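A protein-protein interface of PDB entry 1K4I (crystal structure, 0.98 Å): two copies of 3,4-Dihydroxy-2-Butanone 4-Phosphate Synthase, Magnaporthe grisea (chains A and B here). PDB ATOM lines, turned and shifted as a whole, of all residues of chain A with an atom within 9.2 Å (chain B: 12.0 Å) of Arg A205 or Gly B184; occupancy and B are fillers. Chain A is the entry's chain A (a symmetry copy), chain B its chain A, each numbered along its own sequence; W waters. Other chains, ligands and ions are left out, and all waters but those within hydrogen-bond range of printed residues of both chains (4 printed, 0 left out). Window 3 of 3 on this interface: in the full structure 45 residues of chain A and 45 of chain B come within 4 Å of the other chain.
The backbone carbonyl oxygen (O) of Ala A203 is in hydrogen-bond range of the backbone NH (N) of Leu A208, 2.9 Å away.
Among the printed residues, pairs that only touch across the chains: Trp A206 with Arg B185 (3.4 Å), Trp A206 with Glu B181 (3.5 Å), Phe A56 with Ala B186 (3.5 Å), Phe A56 with Arg B188 (3.5 Å), Phe A56 with Val B187 (3.6 Å), Trp A206 with Val B182 (3.6 Å), Trp A206 with Gly B184 (3.6 Å), Arg A205 with Gly B184 (3.8 Å), Leu A208 with Ala B186 (3.96 Å) and Phe A56 with Arg B185 (3.96 Å).
Val A29 touches none of the printed residues of chain B. No residue of chain B comes within 4 Å of Ala A201. No residue of chain B comes within 4 Å of Phe A202. Of chain B, only Gly B184 (3.8 Å) comes within 4 Å of Arg A205. Gly A207 touches none of the printed residues of chain B. Leu A208 touches just one residue of chain B: Ala B186. Of the printed residues of chain A, Glu B181 touches Trp A206 (3.5 Å). Gly B184 touches just these residues of chain A: Arg A205 and Trp A206. Of the printed residues of chain A, Arg B185 touches Phe A56 and Trp A206. Printed residues of chain A within 4 Å of Ala B186: Phe A56 (3.5 Å) and Leu A208 (3.96 Å). Of the printed residues of chain A, Val B187 touches Phe A56 (3.6 Å). Of the printed residues of chain A, Arg B188 touches Phe A56 (3.5 Å). The nearest residue of chain A that does not touch Gly B184 is Gly A207 (4.4 Å). The nearest printed residue of chain A that does not touch Glu B181 is His A60 (6.5 Å).
Printed residues of chain A that touch a printed residue of chain B: Phe A56, Arg A205, Trp A206 and Leu A208. Of the 10 printed residues of chain B, 7 touch a printed residue of chain A. Hydrophobic or aromatic side chains of chain B that line the printed part of chain A: Ala B186. Along chain B the printed residues that touch a printed residue of chain A span positions 181 to 188.
No position is printed for both chains. Of the 10 pairs that touch across the chains among the printed residues, none has its exchanged pair printed and touching as well.
Water W1 lies within hydrogen-bond range of the backbone carbonyl oxygen (O) of Trp A206 (2.8 Å) and the backbone NH (N) of Ala B186 (3.0 Å). Water W4 lies within hydrogen-bond range of the guanidinium group of Arg B188 (2.8 Å) and a ring nitrogen (NE2) of His A60 (2.8 Å). Water W3 lies within hydrogen-bond range of N of Gly B184 (3.1 Å), O of Arg A205 (3.3 Å) and OE1 of Glu B183 (3.4 Å). Water W2 lies within hydrogen-bond range of O of Arg A205 (3.1 Å) and OE2 of Glu B183 (3.2 Å).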
ATOM      1  N   GLU A  26      13.654 -18.073   6.161  1.00  0.00           N
ATOM      2  CA  GLU A  26      14.969 -18.630   6.432  1.00  0.00           C
ATOM      3  C   GLU A  26      15.747 -18.815   5.147  1.00  0.00           C
ATOM      4  O   GLU A  26      15.206 -18.946   4.053  1.00  0.00           O
ATOM      5  CB  GLU A  26      14.850 -20.048   7.026  1.00  0.00           C
ATOM      6  CG  GLU A  26      13.956 -20.100   8.277  1.00  0.00           C
ATOM      7  CD  GLU A  26      13.961 -21.458   8.940  1.00  0.00           C
ATOM      8  OE1 GLU A  26      14.863 -22.283   8.831  1.00  0.00           O
ATOM      9  OE2 GLU A  26      12.943 -21.618   9.755  1.00  0.00           O
ATOM     10  N   VAL A  29      19.660 -24.177   1.826  1.00  0.00           N
ATOM     11  CA  VAL A  29      20.894 -24.539   1.111  1.00  0.00           C
ATOM     12  C   VAL A  29      20.504 -25.406  -0.087  1.00  0.00           C
ATOM     13  O   VAL A  29      19.852 -26.452   0.103  1.00  0.00           O
ATOM     14  CB  VAL A  29      21.883 -25.242   2.034  1.00  0.00           C
ATOM     15  CG1 VAL A  29      23.122 -25.713   1.261  1.00  0.00           C
ATOM     16  CG2 VAL A  29      22.277 -24.316   3.181  1.00  0.00           C
ATOM     17  N   PHE A  56      25.474 -12.532   7.568  1.00  0.00           N
ATOM     18  CA  PHE A  56      25.802 -13.944   7.594  1.00  0.00           C
ATOM     19  C   PHE A  56      26.055 -14.433   6.168  1.00  0.00           C
ATOM     20  O   PHE A  56      27.000 -15.184   5.895  1.00  0.00           O
ATOM     21  CB  PHE A  56      24.642 -14.728   8.260  1.00  0.00           C
ATOM     22  CG  PHE A  56      24.870 -16.222   8.301  1.00  0.00           C
ATOM     23  CD1 PHE A  56      25.501 -16.815   9.396  1.00  0.00           C
ATOM     24  CD2 PHE A  56      24.458 -17.033   7.235  1.00  0.00           C
ATOM     25  CE1 PHE A  56      25.718 -18.197   9.459  1.00  0.00           C
ATOM     26  CE2 PHE A  56      24.682 -18.413   7.285  1.00  0.00           C
ATOM     27  CZ  PHE A  56      25.302 -18.998   8.392  1.00  0.00           C
ATOM     28  N   HIS A  60      29.648 -16.121   4.794  1.00  0.00           N
ATOM     29  CA  HIS A  60      29.798 -17.514   4.417  1.00  0.00           C
ATOM     30  C   HIS A  60      29.741 -17.799   2.934  1.00  0.00           C
ATOM     31  O   HIS A  60      29.917 -18.951   2.513  1.00  0.00           O
ATOM     32  CB  HIS A  60      28.748 -18.381   5.171  1.00  0.00           C
ATOM     33  CG  HIS A  60      28.993 -18.361   6.636  1.00  0.00           C
ATOM     34  ND1 HIS A  60      30.011 -19.098   7.215  1.00  0.00           N
ATOM     35  CD2 HIS A  60      28.374 -17.643   7.619  1.00  0.00           C
ATOM     36  CE1 HIS A  60      29.980 -18.824   8.530  1.00  0.00           C
ATOM     37  NE2 HIS A  60      29.018 -17.953   8.812  1.00  0.00           N
ATOM     38  N   ILE A 175      28.156 -20.924  -1.664  1.00  0.00           N
ATOM     39  CA  ILE A 175      28.841 -21.215  -0.401  1.00  0.00           C
ATOM     40  C   ILE A 175      30.255 -21.667  -0.731  1.00  0.00           C
ATOM     41  O   ILE A 175      30.487 -22.709  -1.314  1.00  0.00           O
ATOM     42  CB  ILE A 175      28.094 -22.270   0.419  1.00  0.00           C
ATOM     43  CG1 ILE A 175      26.653 -21.807   0.642  1.00  0.00           C
ATOM     44  CG2 ILE A 175      28.823 -22.433   1.755  1.00  0.00           C
ATOM     45  CD1 ILE A 175      25.752 -22.896   1.246  1.00  0.00           C
ATOM     46  N   VAL A 176      31.250 -20.848  -0.359  1.00  0.00           N
ATOM     47  CA  VAL A 176      32.648 -21.196  -0.663  1.00  0.00           C
ATOM     48  C   VAL A 176      33.265 -21.980   0.493  1.00  0.00           C
ATOM     49  O   VAL A 176      32.738 -22.070   1.592  1.00  0.00           O
ATOM     50  CB  VAL A 176      33.470 -19.911  -0.880  1.00  0.00           C
ATOM     51  CG1 VAL A 176      32.926 -19.089  -2.050  1.00  0.00           C
ATOM     52  CG2 VAL A 176      33.565 -19.080   0.401  1.00  0.00           C
ATOM     53  N   ASP A 177      34.434 -22.579   0.203  1.00  0.00           N
ATOM     54  CA  ASP A 177      35.246 -23.209   1.213  1.00  0.00           C
ATOM     55  C   ASP A 177      36.363 -22.174   1.418  1.00  0.00           C
ATOM     56  O   ASP A 177      37.211 -21.965   0.546  1.00  0.00           O
ATOM     57  CB  ASP A 177      35.775 -24.587   0.800  1.00  0.00           C
ATOM     58  CG  ASP A 177      36.659 -25.154   1.903  1.00  0.00           C
ATOM     59  OD1 ASP A 177      37.020 -24.519   2.894  1.00  0.00           O
ATOM     60  OD2 ASP A 177      36.906 -26.429   1.723  1.00  0.00           O
ATOM     61  N   ASP A 178      36.340 -21.481   2.544  1.00  0.00           N
ATOM     62  CA  ASP A 178      37.363 -20.454   2.741  1.00  0.00           C
ATOM     63  C   ASP A 178      38.720 -21.000   3.128  1.00  0.00           C
ATOM     64  O   ASP A 178      39.657 -20.222   3.337  1.00  0.00           O
ATOM     65  CB  ASP A 178      36.932 -19.393   3.739  1.00  0.00           C
ATOM     66  CG  ASP A 178      36.488 -20.059   4.998  1.00  0.00           C
ATOM     67  OD1 ASP A 178      36.812 -21.210   5.271  1.00  0.00           O
ATOM     68  OD2 ASP A 178      35.692 -19.299   5.721  1.00  0.00           O
ATOM     69  N   LEU A 194      32.343 -25.340  -1.359  1.00  0.00           N
ATOM     70  CA  LEU A 194      31.837 -26.400  -0.522  1.00  0.00           C
ATOM     71  C   LEU A 194      31.093 -27.400  -1.385  1.00  0.00           C
ATOM     72  O   LEU A 194      30.336 -27.013  -2.263  1.00  0.00           O
ATOM     73  CB  LEU A 194      30.845 -25.828   0.511  1.00  0.00           C
ATOM     74  CG  LEU A 194      31.001 -26.410   1.901  1.00  0.00           C
ATOM     75  CD1 LEU A 194      32.455 -26.343   2.382  1.00  0.00           C
ATOM     76  CD2 LEU A 194      30.109 -25.672   2.885  1.00  0.00           C
ATOM     77  N   ASP A 197      28.334 -33.509   0.755  1.00  0.00           N
ATOM     78  CA  ASP A 197      28.174 -33.720   2.191  1.00  0.00           C
ATOM     79  C   ASP A 197      28.574 -32.557   3.092  1.00  0.00           C
ATOM     80  O   ASP A 197      28.041 -32.368   4.188  1.00  0.00           O
ATOM     81  CB  ASP A 197      28.886 -34.977   2.675  1.00  0.00           C
ATOM     82  CG  ASP A 197      28.158 -36.221   2.261  1.00  0.00           C
ATOM     83  OD1 ASP A 197      27.008 -36.210   1.830  1.00  0.00           O
ATOM     84  OD2 ASP A 197      28.884 -37.290   2.374  1.00  0.00           O
ATOM     85  N   GLU A 198      29.573 -31.803   2.632  1.00  0.00           N
ATOM     86  CA  GLU A 198      29.985 -30.695   3.431  1.00  0.00           C
ATOM     87  C   GLU A 198      28.896 -29.615   3.450  1.00  0.00           C
ATOM     88  O   GLU A 198      28.785 -28.846   4.423  1.00  0.00           O
ATOM     89  CB  GLU A 198      31.370 -30.192   2.965  1.00  0.00           C
ATOM     90  CG  GLU A 198      31.431 -29.342   1.687  1.00  0.00           C
ATOM     91  CD  GLU A 198      32.756 -29.560   1.003  1.00  0.00           C
ATOM     92  OE1 GLU A 198      33.410 -28.690   0.458  1.00  0.00           O
ATOM     93  OE2 GLU A 198      33.115 -30.815   1.030  1.00  0.00           O
ATOM     94  N   CYS A 199      28.128 -29.547   2.329  1.00  0.00           N
ATOM     95  CA  CYS A 199      27.068 -28.557   2.224  1.00  0.00           C
ATOM     96  C   CYS A 199      25.952 -28.944   3.146  1.00  0.00           C
ATOM     97  O   CYS A 199      25.352 -28.088   3.776  1.00  0.00           O
ATOM     98  CB  CYS A 199      26.580 -28.370   0.793  1.00  0.00           C
ATOM     99  SG  CYS A 199      27.969 -27.793  -0.234  1.00  0.00           S
ATOM    100  N   VAL A 200      25.706 -30.259   3.252  1.00  0.00           N
ATOM    101  CA  VAL A 200      24.682 -30.716   4.160  1.00  0.00           C
ATOM    102  C   VAL A 200      25.114 -30.419   5.588  1.00  0.00           C
ATOM    103  O   VAL A 200      24.318 -29.953   6.433  1.00  0.00           O
ATOM    104  CB  VAL A 200      24.393 -32.204   3.933  1.00  0.00           C
ATOM    105  CG1 VAL A 200      23.469 -32.749   5.047  1.00  0.00           C
ATOM    106  CG2 VAL A 200      23.760 -32.355   2.554  1.00  0.00           C
ATOM    107  N   ALA A 201      26.400 -30.668   5.895  1.00  0.00           N
ATOM    108  CA  ALA A 201      26.872 -30.412   7.233  1.00  0.00           C
ATOM    109  C   ALA A 201      26.773 -28.946   7.599  1.00  0.00           C
ATOM    110  O   ALA A 201      26.474 -28.586   8.730  1.00  0.00           O
ATOM    111  CB  ALA A 201      28.322 -30.907   7.355  1.00  0.00           C
ATOM    112  N   PHE A 202      27.052 -28.073   6.624  1.00  0.00           N
ATOM    113  CA  PHE A 202      26.945 -26.616   6.825  1.00  0.00           C
ATOM    114  C   PHE A 202      25.479 -26.267   7.180  1.00  0.00           C
ATOM    115  O   PHE A 202      25.199 -25.575   8.136  1.00  0.00           O
ATOM    116  CB  PHE A 202      27.344 -25.920   5.501  1.00  0.00           C
ATOM    117  CG  PHE A 202      27.151 -24.423   5.553  1.00  0.00           C
ATOM    118  CD1 PHE A 202      28.167 -23.551   5.958  1.00  0.00           C
ATOM    119  CD2 PHE A 202      25.915 -23.875   5.204  1.00  0.00           C
ATOM    120  CE1 PHE A 202      27.972 -22.172   6.001  1.00  0.00           C
ATOM    121  CE2 PHE A 202      25.699 -22.495   5.230  1.00  0.00           C
ATOM    122  CZ  PHE A 202      26.735 -21.647   5.620  1.00  0.00           C
ATOM    123  N   ALA A 203      24.534 -26.827   6.422  1.00  0.00           N
ATOM    124  CA  ALA A 203      23.133 -26.565   6.698  1.00  0.00           C
ATOM    125  C   ALA A 203      22.779 -26.998   8.111  1.00  0.00           C
ATOM    126  O   ALA A 203      22.101 -26.265   8.843  1.00  0.00           O
ATOM    127  CB  ALA A 203      22.254 -27.265   5.645  1.00  0.00           C
ATOM    128  N   ARG A 204      23.224 -28.196   8.503  1.00  0.00           N
ATOM    129  CA  ARG A 204      22.877 -28.679   9.832  1.00  0.00           C
ATOM    130  C   ARG A 204      23.449 -27.824  10.940  1.00  0.00           C
ATOM    131  O   ARG A 204      22.781 -27.570  11.968  1.00  0.00           O
ATOM    132  CB  ARG A 204      23.286 -30.143  10.023  1.00  0.00           C
ATOM    133  CG  ARG A 204      22.667 -31.117   9.008  1.00  0.00           C
ATOM    134  CD  ARG A 204      21.178 -30.918   8.785  1.00  0.00           C
ATOM    135  NE  ARG A 204      20.612 -31.869   7.810  1.00  0.00           N
ATOM    136  CZ  ARG A 204      19.472 -31.636   7.202  1.00  0.00           C
ATOM    137  NH1 ARG A 204      18.786 -30.517   7.436  1.00  0.00           N
ATOM    138  NH2 ARG A 204      19.026 -32.556   6.343  1.00  0.00           N
ATOM    139  N   ARG A 205      24.702 -27.366  10.765  1.00  0.00           N
ATOM    140  CA  ARG A 205      25.338 -26.521  11.776  1.00  0.00           C
ATOM    141  C   ARG A 205      24.592 -25.208  12.033  1.00  0.00           C
ATOM    142  O   ARG A 205      24.603 -24.630  13.124  1.00  0.00           O
ATOM    143  CB  ARG A 205      26.767 -26.221  11.272  1.00  0.00           C
ATOM    144  CG  ARG A 205      27.555 -25.107  11.943  1.00  0.00           C
ATOM    145  CD  ARG A 205      28.973 -25.045  11.366  1.00  0.00           C
ATOM    146  NE  ARG A 205      29.426 -26.355  10.883  1.00  0.00           N
ATOM    147  CZ  ARG A 205      29.886 -26.676   9.650  1.00  0.00           C
ATOM    148  NH1 ARG A 205      30.079 -25.831   8.642  1.00  0.00           N
ATOM    149  NH2 ARG A 205      30.214 -27.939   9.397  1.00  0.00           N
ATOM    150  N   TRP A 206      23.960 -24.693  10.977  1.00  0.00           N
ATOM    151  CA  TRP A 206      23.290 -23.431  11.051  1.00  0.00           C
ATOM    152  C   TRP A 206      21.772 -23.514  11.139  1.00  0.00           C
ATOM    153  O   TRP A 206      21.106 -22.494  11.025  1.00  0.00           O
ATOM    154  CB  TRP A 206      23.721 -22.556   9.840  1.00  0.00           C
ATOM    155  CG  TRP A 206      25.191 -22.247   9.917  1.00  0.00           C
ATOM    156  CD1 TRP A 206      26.172 -22.671   9.066  1.00  0.00           C
ATOM    157  CD2 TRP A 206      25.837 -21.470  10.930  1.00  0.00           C
ATOM    158  NE1 TRP A 206      27.397 -22.181   9.477  1.00  0.00           N
ATOM    159  CE2 TRP A 206      27.218 -21.463  10.628  1.00  0.00           C
ATOM    160  CE3 TRP A 206      25.378 -20.767  12.034  1.00  0.00           C
ATOM    161  CZ2 TRP A 206      28.150 -20.781  11.405  1.00  0.00           C
ATOM    162  CZ3 TRP A 206      26.301 -20.086  12.801  1.00  0.00           C
ATOM    163  CH2 TRP A 206      27.664 -20.108  12.503  1.00  0.00           C
ATOM    164  N   GLY A 207      21.250 -24.695  11.368  1.00  0.00           N
ATOM    165  CA  GLY A 207      19.787 -24.863  11.520  1.00  0.00           C
ATOM    166  C   GLY A 207      18.995 -24.635  10.242  1.00  0.00           C
ATOM    167  O   GLY A 207      17.837 -24.221  10.330  1.00  0.00           O
ATOM    168  N   LEU A 208      19.574 -24.956   9.084  1.00  0.00           N
ATOM    169  CA  LEU A 208      18.911 -24.708   7.804  1.00  0.00           C
ATOM    170  C   LEU A 208      18.485 -25.963   7.101  1.00  0.00           C
ATOM    171  O   LEU A 208      19.126 -26.999   7.257  1.00  0.00           O
ATOM    172  CB  LEU A 208      19.898 -23.987   6.848  1.00  0.00           C
ATOM    173  CG  LEU A 208      20.574 -22.744   7.449  1.00  0.00           C
ATOM    174  CD1 LEU A 208      21.502 -22.112   6.396  1.00  0.00           C
ATOM    175  CD2 LEU A 208      19.537 -21.707   7.892  1.00  0.00           C
ATOM    176  N   LYS A 209      17.465 -25.849   6.260  1.00  0.00           N
ATOM    177  CA  LYS A 209      17.074 -26.990   5.432  1.00  0.00           C
ATOM    178  C   LYS A 209      18.008 -27.013   4.225  1.00  0.00           C
ATOM    179  O   LYS A 209      18.579 -25.979   3.822  1.00  0.00           O
ATOM    180  CB  LYS A 209      15.630 -26.871   4.958  1.00  0.00           C
ATOM    181  CG  LYS A 209      14.605 -26.809   6.086  1.00  0.00           C
ATOM    182  CD  LYS A 209      14.639 -28.045   6.953  1.00  0.00           C
ATOM    183  CE  LYS A 209      13.665 -27.961   8.122  1.00  0.00           C
ATOM    184  NZ  LYS A 209      13.671 -29.178   8.962  1.00  0.00           N
ATOM    185  N   VAL A 210      18.191 -28.217   3.644  1.00  0.00           N
ATOM    186  CA  VAL A 210      19.099 -28.403   2.520  1.00  0.00           C
ATOM    187  C   VAL A 210      18.447 -29.361   1.517  1.00  0.00           C
ATOM    188  O   VAL A 210      17.769 -30.350   1.888  1.00  0.00           O
ATOM    189  CB  VAL A 210      20.470 -28.899   3.030  1.00  0.00           C
ATOM    190  CG1 VAL A 210      20.351 -30.206   3.829  1.00  0.00           C
ATOM    191  CG2 VAL A 210      21.483 -29.073   1.895  1.00  0.00           C
ATOM    192  N   GLN B 180      29.299 -10.204  14.833  1.00  0.00           N
ATOM    193  CA  GLN B 180      29.616 -11.362  15.638  1.00  0.00           C
ATOM    194  C   GLN B 180      28.797 -12.568  15.269  1.00  0.00           C
ATOM    195  O   GLN B 180      27.609 -12.441  14.953  1.00  0.00           O
ATOM    196  CB  GLN B 180      29.368 -11.086  17.136  1.00  0.00           C
ATOM    197  CG  GLN B 180      30.523 -10.275  17.756  1.00  0.00           C
ATOM    198  CD  GLN B 180      30.377  -8.816  17.417  1.00  0.00           C
ATOM    199  OE1 GLN B 180      31.308  -8.220  16.856  1.00  0.00           O
ATOM    200  NE2 GLN B 180      29.193  -8.247  17.681  1.00  0.00           N
ATOM    201  N   GLU B 181      29.456 -13.706  15.397  1.00  0.00           N
ATOM    202  CA  GLU B 181      28.806 -14.986  15.160  1.00  0.00           C
ATOM    203  C   GLU B 181      27.751 -15.161  16.237  1.00  0.00           C
ATOM    204  O   GLU B 181      27.917 -14.644  17.350  1.00  0.00           O
ATOM    205  CB  GLU B 181      29.835 -16.116  15.320  1.00  0.00           C
ATOM    206  CG  GLU B 181      29.210 -17.500  15.314  1.00  0.00           C
ATOM    207  CD  GLU B 181      30.272 -18.566  15.429  1.00  0.00           C
ATOM    208  OE1 GLU B 181      31.382 -18.318  15.815  1.00  0.00           O
ATOM    209  OE2 GLU B 181      29.901 -19.772  15.122  1.00  0.00           O
ATOM    210  N   VAL B 182      26.670 -15.863  15.874  1.00  0.00           N
ATOM    211  CA  VAL B 182      25.603 -16.181  16.810  1.00  0.00           C
ATOM    212  C   VAL B 182      25.508 -17.689  16.702  1.00  0.00           C
ATOM    213  O   VAL B 182      25.137 -18.212  15.645  1.00  0.00           O
ATOM    214  CB  VAL B 182      24.277 -15.477  16.441  1.00  0.00           C
ATOM    215  CG1 VAL B 182      23.163 -15.962  17.406  1.00  0.00           C
ATOM    216  CG2 VAL B 182      24.445 -13.943  16.479  1.00  0.00           C
ATOM    217  N   GLU B 183      25.888 -18.415  17.774  1.00  0.00           N
ATOM    218  CA  GLU B 183      25.934 -19.869  17.704  1.00  0.00           C
ATOM    219  C   GLU B 183      24.644 -20.485  17.203  1.00  0.00           C
ATOM    220  O   GLU B 183      23.569 -20.187  17.729  1.00  0.00           O
ATOM    221  CB  GLU B 183      26.329 -20.466  19.068  1.00  0.00           C
ATOM    222  CG  GLU B 183      26.218 -22.013  19.125  1.00  0.00           C
ATOM    223  CD  GLU B 183      27.257 -22.703  18.290  1.00  0.00           C
ATOM    224  OE1 GLU B 183      28.128 -22.120  17.667  1.00  0.00           O
ATOM    225  OE2 GLU B 183      27.130 -23.994  18.281  1.00  0.00           O
ATOM    226  N   GLY B 184      24.756 -21.324  16.167  1.00  0.00           N
ATOM    227  CA  GLY B 184      23.583 -22.027  15.639  1.00  0.00           C
ATOM    228  C   GLY B 184      22.549 -21.197  14.899  1.00  0.00           C
ATOM    229  O   GLY B 184      21.513 -21.735  14.563  1.00  0.00           O
ATOM    230  N   ARG B 185      22.809 -19.920  14.610  1.00  0.00           N
ATOM    231  CA  ARG B 185      21.825 -19.083  13.933  1.00  0.00           C
ATOM    232  C   ARG B 185      22.454 -18.431  12.712  1.00  0.00           C
ATOM    233  O   ARG B 185      23.583 -17.927  12.786  1.00  0.00           O
ATOM    234  CB  ARG B 185      21.332 -17.973  14.867  1.00  0.00           C
ATOM    235  CG  ARG B 185      20.791 -18.485  16.210  1.00  0.00           C
ATOM    236  CD  ARG B 185      19.451 -19.195  16.065  1.00  0.00           C
ATOM    237  NE  ARG B 185      18.988 -19.584  17.393  1.00  0.00           N
ATOM    238  CZ  ARG B 185      18.115 -20.567  17.573  1.00  0.00           C
ATOM    239  NH1 ARG B 185      17.576 -21.199  16.517  1.00  0.00           N
ATOM    240  NH2 ARG B 185      17.770 -20.882  18.846  1.00  0.00           N
ATOM    241  N   ALA B 186      21.698 -18.387  11.618  1.00  0.00           N
ATOM    242  CA  ALA B 186      22.170 -17.819  10.376  1.00  0.00           C
ATOM    243  C   ALA B 186      22.030 -16.302  10.302  1.00  0.00           C
ATOM    244  O   ALA B 186      21.400 -15.752   9.410  1.00  0.00           O
ATOM    245  CB  ALA B 186      21.519 -18.534   9.177  1.00  0.00           C
ATOM    246  N   VAL B 187      22.693 -15.639  11.265  1.00  0.00           N
ATOM    247  CA  VAL B 187      22.719 -14.178  11.358  1.00  0.00           C
ATOM    248  C   VAL B 187      24.073 -13.795  11.939  1.00  0.00           C
ATOM    249  O   VAL B 187      24.731 -14.622  12.569  1.00  0.00           O
ATOM    250  CB  VAL B 187      21.660 -13.602  12.326  1.00  0.00           C
ATOM    251  CG1 VAL B 187      20.244 -13.782  11.736  1.00  0.00           C
ATOM    252  CG2 VAL B 187      21.766 -14.225  13.727  1.00  0.00           C
ATOM    253  N   ARG B 188      24.475 -12.539  11.766  1.00  0.00           N
ATOM    254  CA  ARG B 188      25.665 -12.007  12.446  1.00  0.00           C
ATOM    255  C   ARG B 188      25.174 -10.726  13.121  1.00  0.00           C
ATOM    256  O   ARG B 188      24.538  -9.886  12.478  1.00  0.00           O
ATOM    257  CB  ARG B 188      26.826 -11.575  11.545  1.00  0.00           C
ATOM    258  CG  ARG B 188      27.293 -12.614  10.570  1.00  0.00           C
ATOM    259  CD  ARG B 188      28.269 -13.578  11.162  1.00  0.00           C
ATOM    260  NE  ARG B 188      29.503 -12.927  11.594  1.00  0.00           N
ATOM    261  CZ  ARG B 188      30.558 -13.643  11.967  1.00  0.00           C
ATOM    262  NH1 ARG B 188      30.545 -14.979  11.892  1.00  0.00           N
ATOM    263  NH2 ARG B 188      31.642 -12.978  12.415  1.00  0.00           N
ATOM    264  N   ALA B 189      25.502 -10.545  14.373  1.00  0.00           N
ATOM    265  CA  ALA B 189      25.050  -9.337  15.081  1.00  0.00           C
ATOM    266  C   ALA B 189      25.973  -8.159  14.873  1.00  0.00           C
ATOM    267  O   ALA B 189      27.196  -8.317  14.799  1.00  0.00           O
ATOM    268  CB  ALA B 189      25.021  -9.631  16.576  1.00  0.00           C
HETATM  269  O   HOH W   1      19.422 -20.382  11.629  1.00  0.00           O
HETATM  270  O   HOH W   2      26.483 -25.500  15.477  1.00  0.00           O
HETATM  271  O   HOH W   3      26.885 -22.825  14.580  1.00  0.00           O
HETATM  272  O   HOH W   4      28.638 -16.997  11.456  1.00  0.00           O
